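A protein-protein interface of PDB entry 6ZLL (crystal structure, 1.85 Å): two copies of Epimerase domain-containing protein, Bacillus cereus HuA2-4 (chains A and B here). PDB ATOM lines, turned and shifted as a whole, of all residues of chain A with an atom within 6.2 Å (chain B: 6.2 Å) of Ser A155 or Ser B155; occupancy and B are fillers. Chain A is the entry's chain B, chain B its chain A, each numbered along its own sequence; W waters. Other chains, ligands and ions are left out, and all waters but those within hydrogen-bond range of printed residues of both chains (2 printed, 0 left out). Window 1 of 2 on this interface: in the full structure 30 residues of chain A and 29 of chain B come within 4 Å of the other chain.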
ATOM      1  N   PHE A  95      18.944  10.717  -1.293  1.00  0.00           N
ATOM      2  CA  PHE A  95      18.005  10.068  -0.333  1.00  0.00           C
ATOM      3  C   PHE A  95      16.973  11.062   0.203  1.00  0.00           C
ATOM      4  O   PHE A  95      15.807  10.692   0.283  1.00  0.00           O
ATOM      5  CB  PHE A  95      18.752   9.417   0.818  1.00  0.00           C
ATOM      6  CG  PHE A  95      17.886   8.658   1.797  1.00  0.00           C
ATOM      7  CD1 PHE A  95      17.160   7.556   1.400  1.00  0.00           C
ATOM      8  CD2 PHE A  95      17.870   8.996   3.139  1.00  0.00           C
ATOM      9  CE1 PHE A  95      16.401   6.833   2.311  1.00  0.00           C
ATOM     10  CE2 PHE A  95      17.090   8.290   4.048  1.00  0.00           C
ATOM     11  CZ  PHE A  95      16.386   7.190   3.633  1.00  0.00           C
ATOM     12  N   ASN A 102       8.086  10.635   0.427  1.00  0.00           N
ATOM     13  CA  ASN A 102       7.504   9.289   0.664  1.00  0.00           C
ATOM     14  C   ASN A 102       7.090   9.155   2.131  1.00  0.00           C
ATOM     15  O   ASN A 102       6.218   8.302   2.381  1.00  0.00           O
ATOM     16  CB  ASN A 102       8.449   8.155   0.287  1.00  0.00           C
ATOM     17  CG  ASN A 102       8.783   8.108  -1.182  1.00  0.00           C
ATOM     18  OD1 ASN A 102       8.143   8.786  -1.972  1.00  0.00           O
ATOM     19  ND2 ASN A 102       9.798   7.338  -1.558  1.00  0.00           N
ATOM     20  N   ILE A 103       7.760   9.877   3.051  1.00  0.00           N
ATOM     21  CA  ILE A 103       7.459   9.792   4.514  1.00  0.00           C
ATOM     22  C   ILE A 103       6.699  11.047   4.950  1.00  0.00           C
ATOM     23  O   ILE A 103       5.533  10.874   5.401  1.00  0.00           O
ATOM     24  CB  ILE A 103       8.728   9.518   5.344  1.00  0.00           C
ATOM     25  CG1 ILE A 103       9.461   8.274   4.850  1.00  0.00           C
ATOM     26  CG2 ILE A 103       8.358   9.409   6.809  1.00  0.00           C
ATOM     27  CD1 ILE A 103      10.718   7.909   5.625  1.00  0.00           C
ATOM     28  N   THR A 106       3.199  11.489   3.184  1.00  0.00           N
ATOM     29  CA  THR A 106       2.242  10.479   3.686  1.00  0.00           C
ATOM     30  C   THR A 106       1.748  10.903   5.063  1.00  0.00           C
ATOM     31  O   THR A 106       0.521  10.934   5.263  1.00  0.00           O
ATOM     32  CB  THR A 106       2.863   9.077   3.675  1.00  0.00           C
ATOM     33  OG1 THR A 106       3.182   8.849   2.302  1.00  0.00           O
ATOM     34  CG2 THR A 106       1.925   7.998   4.180  1.00  0.00           C
ATOM     35  N   GLY A 150      12.913   1.480  -0.922  1.00  0.00           N
ATOM     36  CA  GLY A 150      12.061   0.469  -0.276  1.00  0.00           C
ATOM     37  C   GLY A 150      11.841   0.793   1.188  1.00  0.00           C
ATOM     38  O   GLY A 150      10.718   0.647   1.668  1.00  0.00           O
ATOM     39  N   VAL A 151      12.880   1.263   1.876  1.00  0.00           N
ATOM     40  CA  VAL A 151      12.718   1.680   3.291  1.00  0.00           C
ATOM     41  C   VAL A 151      11.682   2.809   3.403  1.00  0.00           C
ATOM     42  O   VAL A 151      10.799   2.721   4.285  1.00  0.00           O
ATOM     43  CB  VAL A 151      14.063   2.113   3.865  1.00  0.00           C
ATOM     44  CG1 VAL A 151      13.887   2.681   5.264  1.00  0.00           C
ATOM     45  CG2 VAL A 151      15.055   0.965   3.854  1.00  0.00           C
ATOM     46  N   THR A 152      11.818   3.880   2.616  1.00  0.00           N
ATOM     47  CA  THR A 152      10.922   5.048   2.719  1.00  0.00           C
ATOM     48  C   THR A 152       9.504   4.585   2.390  1.00  0.00           C
ATOM     49  O   THR A 152       8.562   5.137   2.962  1.00  0.00           O
ATOM     50  CB  THR A 152      11.353   6.278   1.899  1.00  0.00           C
ATOM     51  OG1 THR A 152      11.277   5.986   0.511  1.00  0.00           O
ATOM     52  CG2 THR A 152      12.737   6.795   2.239  1.00  0.00           C
ATOM     53  N   LYS A 153       9.337   3.656   1.460  1.00  0.00           N
ATOM     54  CA  LYS A 153       7.978   3.251   1.034  1.00  0.00           C
ATOM     55  C   LYS A 153       7.359   2.392   2.131  1.00  0.00           C
ATOM     56  O   LYS A 153       6.169   2.644   2.443  1.00  0.00           O
ATOM     57  CB  LYS A 153       8.003   2.577  -0.331  1.00  0.00           C
ATOM     58  CG  LYS A 153       8.255   3.585  -1.451  1.00  0.00           C
ATOM     59  CD  LYS A 153       7.119   4.566  -1.680  1.00  0.00           C
ATOM     60  CE  LYS A 153       5.926   3.864  -2.291  1.00  0.00           C
ATOM     61  NZ  LYS A 153       4.827   4.810  -2.613  1.00  0.00           N
ATOM     62  N   LEU A 154       8.171   1.583   2.804  1.00  0.00           N
ATOM     63  CA  LEU A 154       7.679   0.730   3.930  1.00  0.00           C
ATOM     64  C   LEU A 154       7.277   1.630   5.106  1.00  0.00           C
ATOM     65  O   LEU A 154       6.290   1.326   5.807  1.00  0.00           O
ATOM     66  CB  LEU A 154       8.779  -0.266   4.282  1.00  0.00           C
ATOM     67  CG  LEU A 154       8.480  -1.239   5.414  1.00  0.00           C
ATOM     68  CD1 LEU A 154       7.165  -1.956   5.189  1.00  0.00           C
ATOM     69  CD2 LEU A 154       9.627  -2.237   5.525  1.00  0.00           C
ATOM     70  N   SER A 155       8.021   2.720   5.304  1.00  0.00           N
ATOM     71  CA  SER A 155       7.774   3.764   6.322  1.00  0.00           C
ATOM     72  C   SER A 155       6.399   4.419   6.071  1.00  0.00           C
ATOM     73  O   SER A 155       5.688   4.655   7.054  1.00  0.00           O
ATOM     74  CB  SER A 155       8.920   4.727   6.296  1.00  0.00           C
ATOM     75  OG  SER A 155       9.069   5.416   7.517  1.00  0.00           O
ATOM     76  N   GLY A 156       6.018   4.666   4.807  1.00  0.00           N
ATOM     77  CA  GLY A 156       4.672   5.165   4.452  1.00  0.00           C
ATOM     78  C   GLY A 156       3.579   4.160   4.828  1.00  0.00           C
ATOM     79  O   GLY A 156       2.541   4.586   5.349  1.00  0.00           O
ATOM     80  N   GLU A 157       3.783   2.879   4.538  1.00  0.00           N
ATOM     81  CA  GLU A 157       2.843   1.778   4.901  1.00  0.00           C
ATOM     82  C   GLU A 157       2.640   1.803   6.410  1.00  0.00           C
ATOM     83  O   GLU A 157       1.507   1.827   6.844  1.00  0.00           O
ATOM     84  CB  GLU A 157       3.376   0.389   4.552  1.00  0.00           C
ATOM     85  CG  GLU A 157       3.446   0.109   3.057  1.00  0.00           C
ATOM     86  CD  GLU A 157       3.607  -1.370   2.716  1.00  0.00           C
ATOM     87  OE1 GLU A 157       3.332  -2.240   3.614  1.00  0.00           O
ATOM     88  OE2 GLU A 157       3.977  -1.654   1.576  1.00  0.00           O
ATOM     89  N   HIS A 158       3.739   1.844   7.151  1.00  0.00           N
ATOM     90  CA  HIS A 158       3.716   1.874   8.643  1.00  0.00           C
ATOM     91  C   HIS A 158       2.924   3.088   9.155  1.00  0.00           C
ATOM     92  O   HIS A 158       2.173   2.925  10.144  1.00  0.00           O
ATOM     93  CB  HIS A 158       5.142   1.863   9.182  1.00  0.00           C
ATOM     94  CG  HIS A 158       5.814   0.555   8.989  1.00  0.00           C
ATOM     95  ND1 HIS A 158       7.172   0.454   8.870  1.00  0.00           N
ATOM     96  CD2 HIS A 158       5.314  -0.701   8.905  1.00  0.00           C
ATOM     97  CE1 HIS A 158       7.485  -0.832   8.726  1.00  0.00           C
ATOM     98  NE2 HIS A 158       6.368  -1.544   8.720  1.00  0.00           N
ATOM     99  N   LEU A 159       3.144   4.276   8.584  1.00  0.00           N
ATOM    100  CA  LEU A 159       2.347   5.478   8.924  1.00  0.00           C
ATOM    101  C   LEU A 159       0.873   5.151   8.663  1.00  0.00           C
ATOM    102  O   LEU A 159       0.062   5.517   9.491  1.00  0.00           O
ATOM    103  CB  LEU A 159       2.789   6.706   8.117  1.00  0.00           C
ATOM    104  CG  LEU A 159       4.145   7.300   8.490  1.00  0.00           C
ATOM    105  CD1 LEU A 159       4.613   8.296   7.440  1.00  0.00           C
ATOM    106  CD2 LEU A 159       4.093   7.943   9.869  1.00  0.00           C
ATOM    107  N   CYS A 160       0.509   4.479   7.569  1.00  0.00           N
ATOM    108  CA  CYS A 160      -0.917   4.162   7.332  1.00  0.00           C
ATOM    109  C   CYS A 160      -1.464   3.337   8.503  1.00  0.00           C
ATOM    110  O   CYS A 160      -2.574   3.632   8.931  1.00  0.00           O
ATOM    111  CB  CYS A 160      -1.139   3.429   6.016  1.00  0.00           C
ATOM    112  SG  CYS A 160      -0.789   4.518   4.621  1.00  0.00           S
ATOM    113  N   ASN B 102      16.093  10.757  13.366  1.00  0.00           N
ATOM    114  CA  ASN B 102      16.008   9.278  13.497  1.00  0.00           C
ATOM    115  C   ASN B 102      16.320   8.653  12.142  1.00  0.00           C
ATOM    116  O   ASN B 102      16.988   7.612  12.146  1.00  0.00           O
ATOM    117  CB  ASN B 102      14.673   8.799  14.073  1.00  0.00           C
ATOM    118  CG  ASN B 102      14.403   9.341  15.454  1.00  0.00           C
ATOM    119  OD1 ASN B 102      15.284   9.963  16.046  1.00  0.00           O
ATOM    120  ND2 ASN B 102      13.196   9.141  15.972  1.00  0.00           N
ATOM    121  N   ILE B 103      15.856   9.241  11.029  1.00  0.00           N
ATOM    122  CA  ILE B 103      16.014   8.633   9.676  1.00  0.00           C
ATOM    123  C   ILE B 103      17.216   9.245   8.936  1.00  0.00           C
ATOM    124  O   ILE B 103      18.154   8.463   8.610  1.00  0.00           O
ATOM    125  CB  ILE B 103      14.711   8.754   8.876  1.00  0.00           C
ATOM    126  CG1 ILE B 103      13.556   8.101   9.640  1.00  0.00           C
ATOM    127  CG2 ILE B 103      14.872   8.147   7.490  1.00  0.00           C
ATOM    128  CD1 ILE B 103      12.293   8.013   8.831  1.00  0.00           C
ATOM    129  N   THR B 106      20.616   8.614  10.741  1.00  0.00           N
ATOM    130  CA  THR B 106      21.041   7.211  10.627  1.00  0.00           C
ATOM    131  C   THR B 106      21.587   7.005   9.201  1.00  0.00           C
ATOM    132  O   THR B 106      22.662   6.405   9.044  1.00  0.00           O
ATOM    133  CB  THR B 106      19.923   6.248  11.036  1.00  0.00           C
ATOM    134  OG1 THR B 106      19.560   6.537  12.385  1.00  0.00           O
ATOM    135  CG2 THR B 106      20.354   4.804  10.915  1.00  0.00           C
ATOM    136  N   VAL B 129       8.919  -0.170  17.987  1.00  0.00           N
ATOM    137  CA  VAL B 129       8.806  -0.733  16.610  1.00  0.00           C
ATOM    138  C   VAL B 129       7.754  -1.862  16.581  1.00  0.00           C
ATOM    139  O   VAL B 129       7.151  -2.040  15.514  1.00  0.00           O
ATOM    140  CB  VAL B 129      10.162  -1.177  16.026  1.00  0.00           C
ATOM    141  CG1 VAL B 129      11.188  -0.061  16.081  1.00  0.00           C
ATOM    142  CG2 VAL B 129      10.693  -2.462  16.645  1.00  0.00           C
ATOM    143  N   GLY B 150       7.794   5.255  16.634  1.00  0.00           N
ATOM    144  CA  GLY B 150       8.048   3.843  16.299  1.00  0.00           C
ATOM    145  C   GLY B 150       8.389   3.656  14.837  1.00  0.00           C
ATOM    146  O   GLY B 150       9.411   2.988  14.540  1.00  0.00           O
ATOM    147  N   VAL B 151       7.603   4.251  13.951  1.00  0.00           N
ATOM    148  CA  VAL B 151       7.876   4.248  12.475  1.00  0.00           C
ATOM    149  C   VAL B 151       9.284   4.760  12.165  1.00  0.00           C
ATOM    150  O   VAL B 151       9.990   4.064  11.405  1.00  0.00           O
ATOM    151  CB  VAL B 151       6.832   5.081  11.724  1.00  0.00           C
ATOM    152  CG1 VAL B 151       7.152   5.120  10.240  1.00  0.00           C
ATOM    153  CG2 VAL B 151       5.434   4.541  11.976  1.00  0.00           C
ATOM    154  N   THR B 152       9.678   5.926  12.704  1.00  0.00           N
ATOM    155  CA  THR B 152      10.999   6.542  12.404  1.00  0.00           C
ATOM    156  C   THR B 152      12.126   5.619  12.897  1.00  0.00           C
ATOM    157  O   THR B 152      13.105   5.440  12.164  1.00  0.00           O
ATOM    158  CB  THR B 152      11.105   7.972  12.933  1.00  0.00           C
ATOM    159  OG1 THR B 152      11.085   8.049  14.370  1.00  0.00           O
ATOM    160  CG2 THR B 152      10.021   8.824  12.319  1.00  0.00           C
ATOM    161  N   LYS B 153      11.955   4.979  14.047  1.00  0.00           N
ATOM    162  CA  LYS B 153      12.995   4.085  14.612  1.00  0.00           C
ATOM    163  C   LYS B 153      13.035   2.795  13.793  1.00  0.00           C
ATOM    164  O   LYS B 153      14.138   2.335  13.516  1.00  0.00           O
ATOM    165  CB  LYS B 153      12.731   3.881  16.098  1.00  0.00           C
ATOM    166  CG  LYS B 153      12.937   5.147  16.903  1.00  0.00           C
ATOM    167  CD  LYS B 153      14.409   5.499  17.034  1.00  0.00           C
ATOM    168  CE  LYS B 153      15.170   4.456  17.828  1.00  0.00           C
ATOM    169  NZ  LYS B 153      16.542   4.906  18.152  1.00  0.00           N
ATOM    170  N   LEU B 154      11.888   2.268  13.356  1.00  0.00           N
ATOM    171  CA  LEU B 154      11.878   1.052  12.510  1.00  0.00           C
ATOM    172  C   LEU B 154      12.548   1.354  11.161  1.00  0.00           C
ATOM    173  O   LEU B 154      13.318   0.491  10.651  1.00  0.00           O
ATOM    174  CB  LEU B 154      10.449   0.550  12.345  1.00  0.00           C
ATOM    175  CG  LEU B 154      10.296  -0.786  11.628  1.00  0.00           C
ATOM    176  CD1 LEU B 154      11.268  -1.842  12.139  1.00  0.00           C
ATOM    177  CD2 LEU B 154       8.868  -1.285  11.741  1.00  0.00           C
ATOM    178  N   SER B 155      12.334   2.566  10.644  1.00  0.00           N
ATOM    179  CA  SER B 155      12.995   3.059   9.403  1.00  0.00           C
ATOM    180  C   SER B 155      14.525   3.051   9.602  1.00  0.00           C
ATOM    181  O   SER B 155      15.247   2.612   8.717  1.00  0.00           O
ATOM    182  CB  SER B 155      12.461   4.410   9.026  1.00  0.00           C
ATOM    183  OG  SER B 155      12.684   4.646   7.650  1.00  0.00           O
ATOM    184  N   GLY B 156      15.015   3.458  10.766  1.00  0.00           N
ATOM    185  CA  GLY B 156      16.464   3.410  11.066  1.00  0.00           C
ATOM    186  C   GLY B 156      16.992   1.994  11.013  1.00  0.00           C
ATOM    187  O   GLY B 156      18.104   1.784  10.490  1.00  0.00           O
ATOM    188  N   GLU B 157      16.253   1.064  11.605  1.00  0.00           N
ATOM    189  CA  GLU B 157      16.593  -0.373  11.612  1.00  0.00           C
ATOM    190  C   GLU B 157      16.681  -0.856  10.169  1.00  0.00           C
ATOM    191  O   GLU B 157      17.670  -1.511   9.831  1.00  0.00           O
ATOM    192  CB  GLU B 157      15.566  -1.250  12.310  1.00  0.00           C
ATOM    193  CG  GLU B 157      15.429  -1.033  13.798  1.00  0.00           C
ATOM    194  CD  GLU B 157      14.687  -2.174  14.509  1.00  0.00           C
ATOM    195  OE1 GLU B 157      14.576  -3.268  13.909  1.00  0.00           O
ATOM    196  OE2 GLU B 157      14.231  -1.979  15.678  1.00  0.00           O
ATOM    197  N   HIS B 158      15.694  -0.517   9.338  1.00  0.00           N
ATOM    198  CA  HIS B 158      15.704  -0.986   7.924  1.00  0.00           C
ATOM    199  C   HIS B 158      16.898  -0.399   7.184  1.00  0.00           C
ATOM    200  O   HIS B 158      17.431  -1.113   6.321  1.00  0.00           O
ATOM    201  CB  HIS B 158      14.382  -0.668   7.212  1.00  0.00           C
ATOM    202  CG  HIS B 158      13.282  -1.555   7.673  1.00  0.00           C
ATOM    203  ND1 HIS B 158      12.105  -1.067   8.179  1.00  0.00           N
ATOM    204  CD2 HIS B 158      13.199  -2.897   7.743  1.00  0.00           C
ATOM    205  CE1 HIS B 158      11.340  -2.078   8.522  1.00  0.00           C
ATOM    206  NE2 HIS B 158      11.991  -3.190   8.293  1.00  0.00           N
ATOM    207  N   LEU B 159      17.279   0.854   7.467  1.00  0.00           N
ATOM    208  CA  LEU B 159      18.469   1.490   6.841  1.00  0.00           C
ATOM    209  C   LEU B 159      19.716   0.690   7.244  1.00  0.00           C
ATOM    210  O   LEU B 159      20.503   0.360   6.352  1.00  0.00           O
ATOM    211  CB  LEU B 159      18.581   2.975   7.244  1.00  0.00           C
ATOM    212  CG  LEU B 159      17.645   3.939   6.509  1.00  0.00           C
ATOM    213  CD1 LEU B 159      17.633   5.306   7.173  1.00  0.00           C
ATOM    214  CD2 LEU B 159      18.027   4.064   5.043  1.00  0.00           C
ATOM    215  N   CYS B 160      19.861   0.330   8.524  1.00  0.00           N
ATOM    216  CA  CYS B 160      20.931  -0.602   8.990  1.00  0.00           C
ATOM    217  C   CYS B 160      20.979  -1.872   8.128  1.00  0.00           C
ATOM    218  O   CYS B 160      22.081  -2.221   7.635  1.00  0.00           O
ATOM    219  CB  CYS B 160      20.769  -0.940  10.465  1.00  0.00           C
ATOM    220  SG  CYS B 160      21.162   0.495  11.486  1.00  0.00           S
HETATM  221  O   HOH W   1       9.366   2.250   9.085  1.00  0.00           O
HETATM  222  O   HOH W   2      10.998   1.525   6.964  1.00  0.00           O
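A ring nitrogen (ND1) of His B158 lies within hydrogen-bond range of the backbone carbonyl oxygen of Leu B154.
O of Leu A154 is in hydrogen-bond range of ND1 of His A158 (3.3 Å).
Phe A95 touches Leu B159 (CZ to CD2, 3.8 Å).
Ile B103 touches Ile A103 (CD1 to CD1, 3.6 Å).
Ser B155 touches Val A151 (OG to CG1, 3.3 Å).
Val A151 touches His B158 (CG2 to CB, 3.8 Å).
His B158 touches Leu A154.
Ser A155 touches Val B151 (OG to CG1, 3.3 Å).
OG of Ser B155 touches OG of Ser A155, 3.7 Å away.
His A158 touches Val B151.
Leu B154 touches His A158 (CD2 to CE1, 3.3 Å).
Printed residues of chain B within 4 Å of Leu A154: His B158.
Of chain B, only Val B151 and Ser B155 come within 4 Å of Ser A155.
Leu A159 touches none of the printed residues of chain B.
Of the printed residues of chain A, Val B151 touches Ser A155 (3.3 Å) and His A158 (3.9 Å).
Of chain A, only Val A151 and Ser A155 come within 4 Å of Ser B155.
Glu B157 touches none of the printed residues of chain A.
Of the 15 printed residues of chain A, 6 touch a printed residue of chain B.
Printed residues of chain A that touch a printed residue of chain B: Phe A95, Ile A103, Val A151, Leu A154, Ser A155 and His A158.
Hydrophobic or aromatic side chains of chain A within 4 Å of the printed part of chain B: Phe A95, Ile A103, Val A151, Leu A154 and His A158.
Of the 15 printed residues of chain B, 6 touch a printed residue of chain A.
Hydrophobic or aromatic side chains of chain B within 4 Å of the printed part of chain A: Ile B103, Val B151, Leu B154, His B158 and Leu B159.
Among the printed residues, 9 pairs touch across the chains.
Ile A103 touches its own counterpart, Ile B103.
Val A151 touches Ser B155, and with the chains exchanged Ser A155 touches Val B151.
Val A151 touches His B158, and with the chains exchanged His A158 touches Val B151.
Leu A154 touches His B158, and with the chains exchanged His A158 touches Leu B154.
Of the 9 pairs that touch across the chains among the printed residues, 8 have their exchanged pair printed and touching as well.
Water W1 lies within hydrogen-bond range of a ring nitrogen (ND1) of His A158 (2.8 Å), the backbone carbonyl oxygen of Val B151 (3.0 Å) and the backbone NH of Ser B155 (3.4 Å).
Water W2 bridges the backbone carbonyl oxygen of Val A151 and a ring nitrogen (ND1) of His B158.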
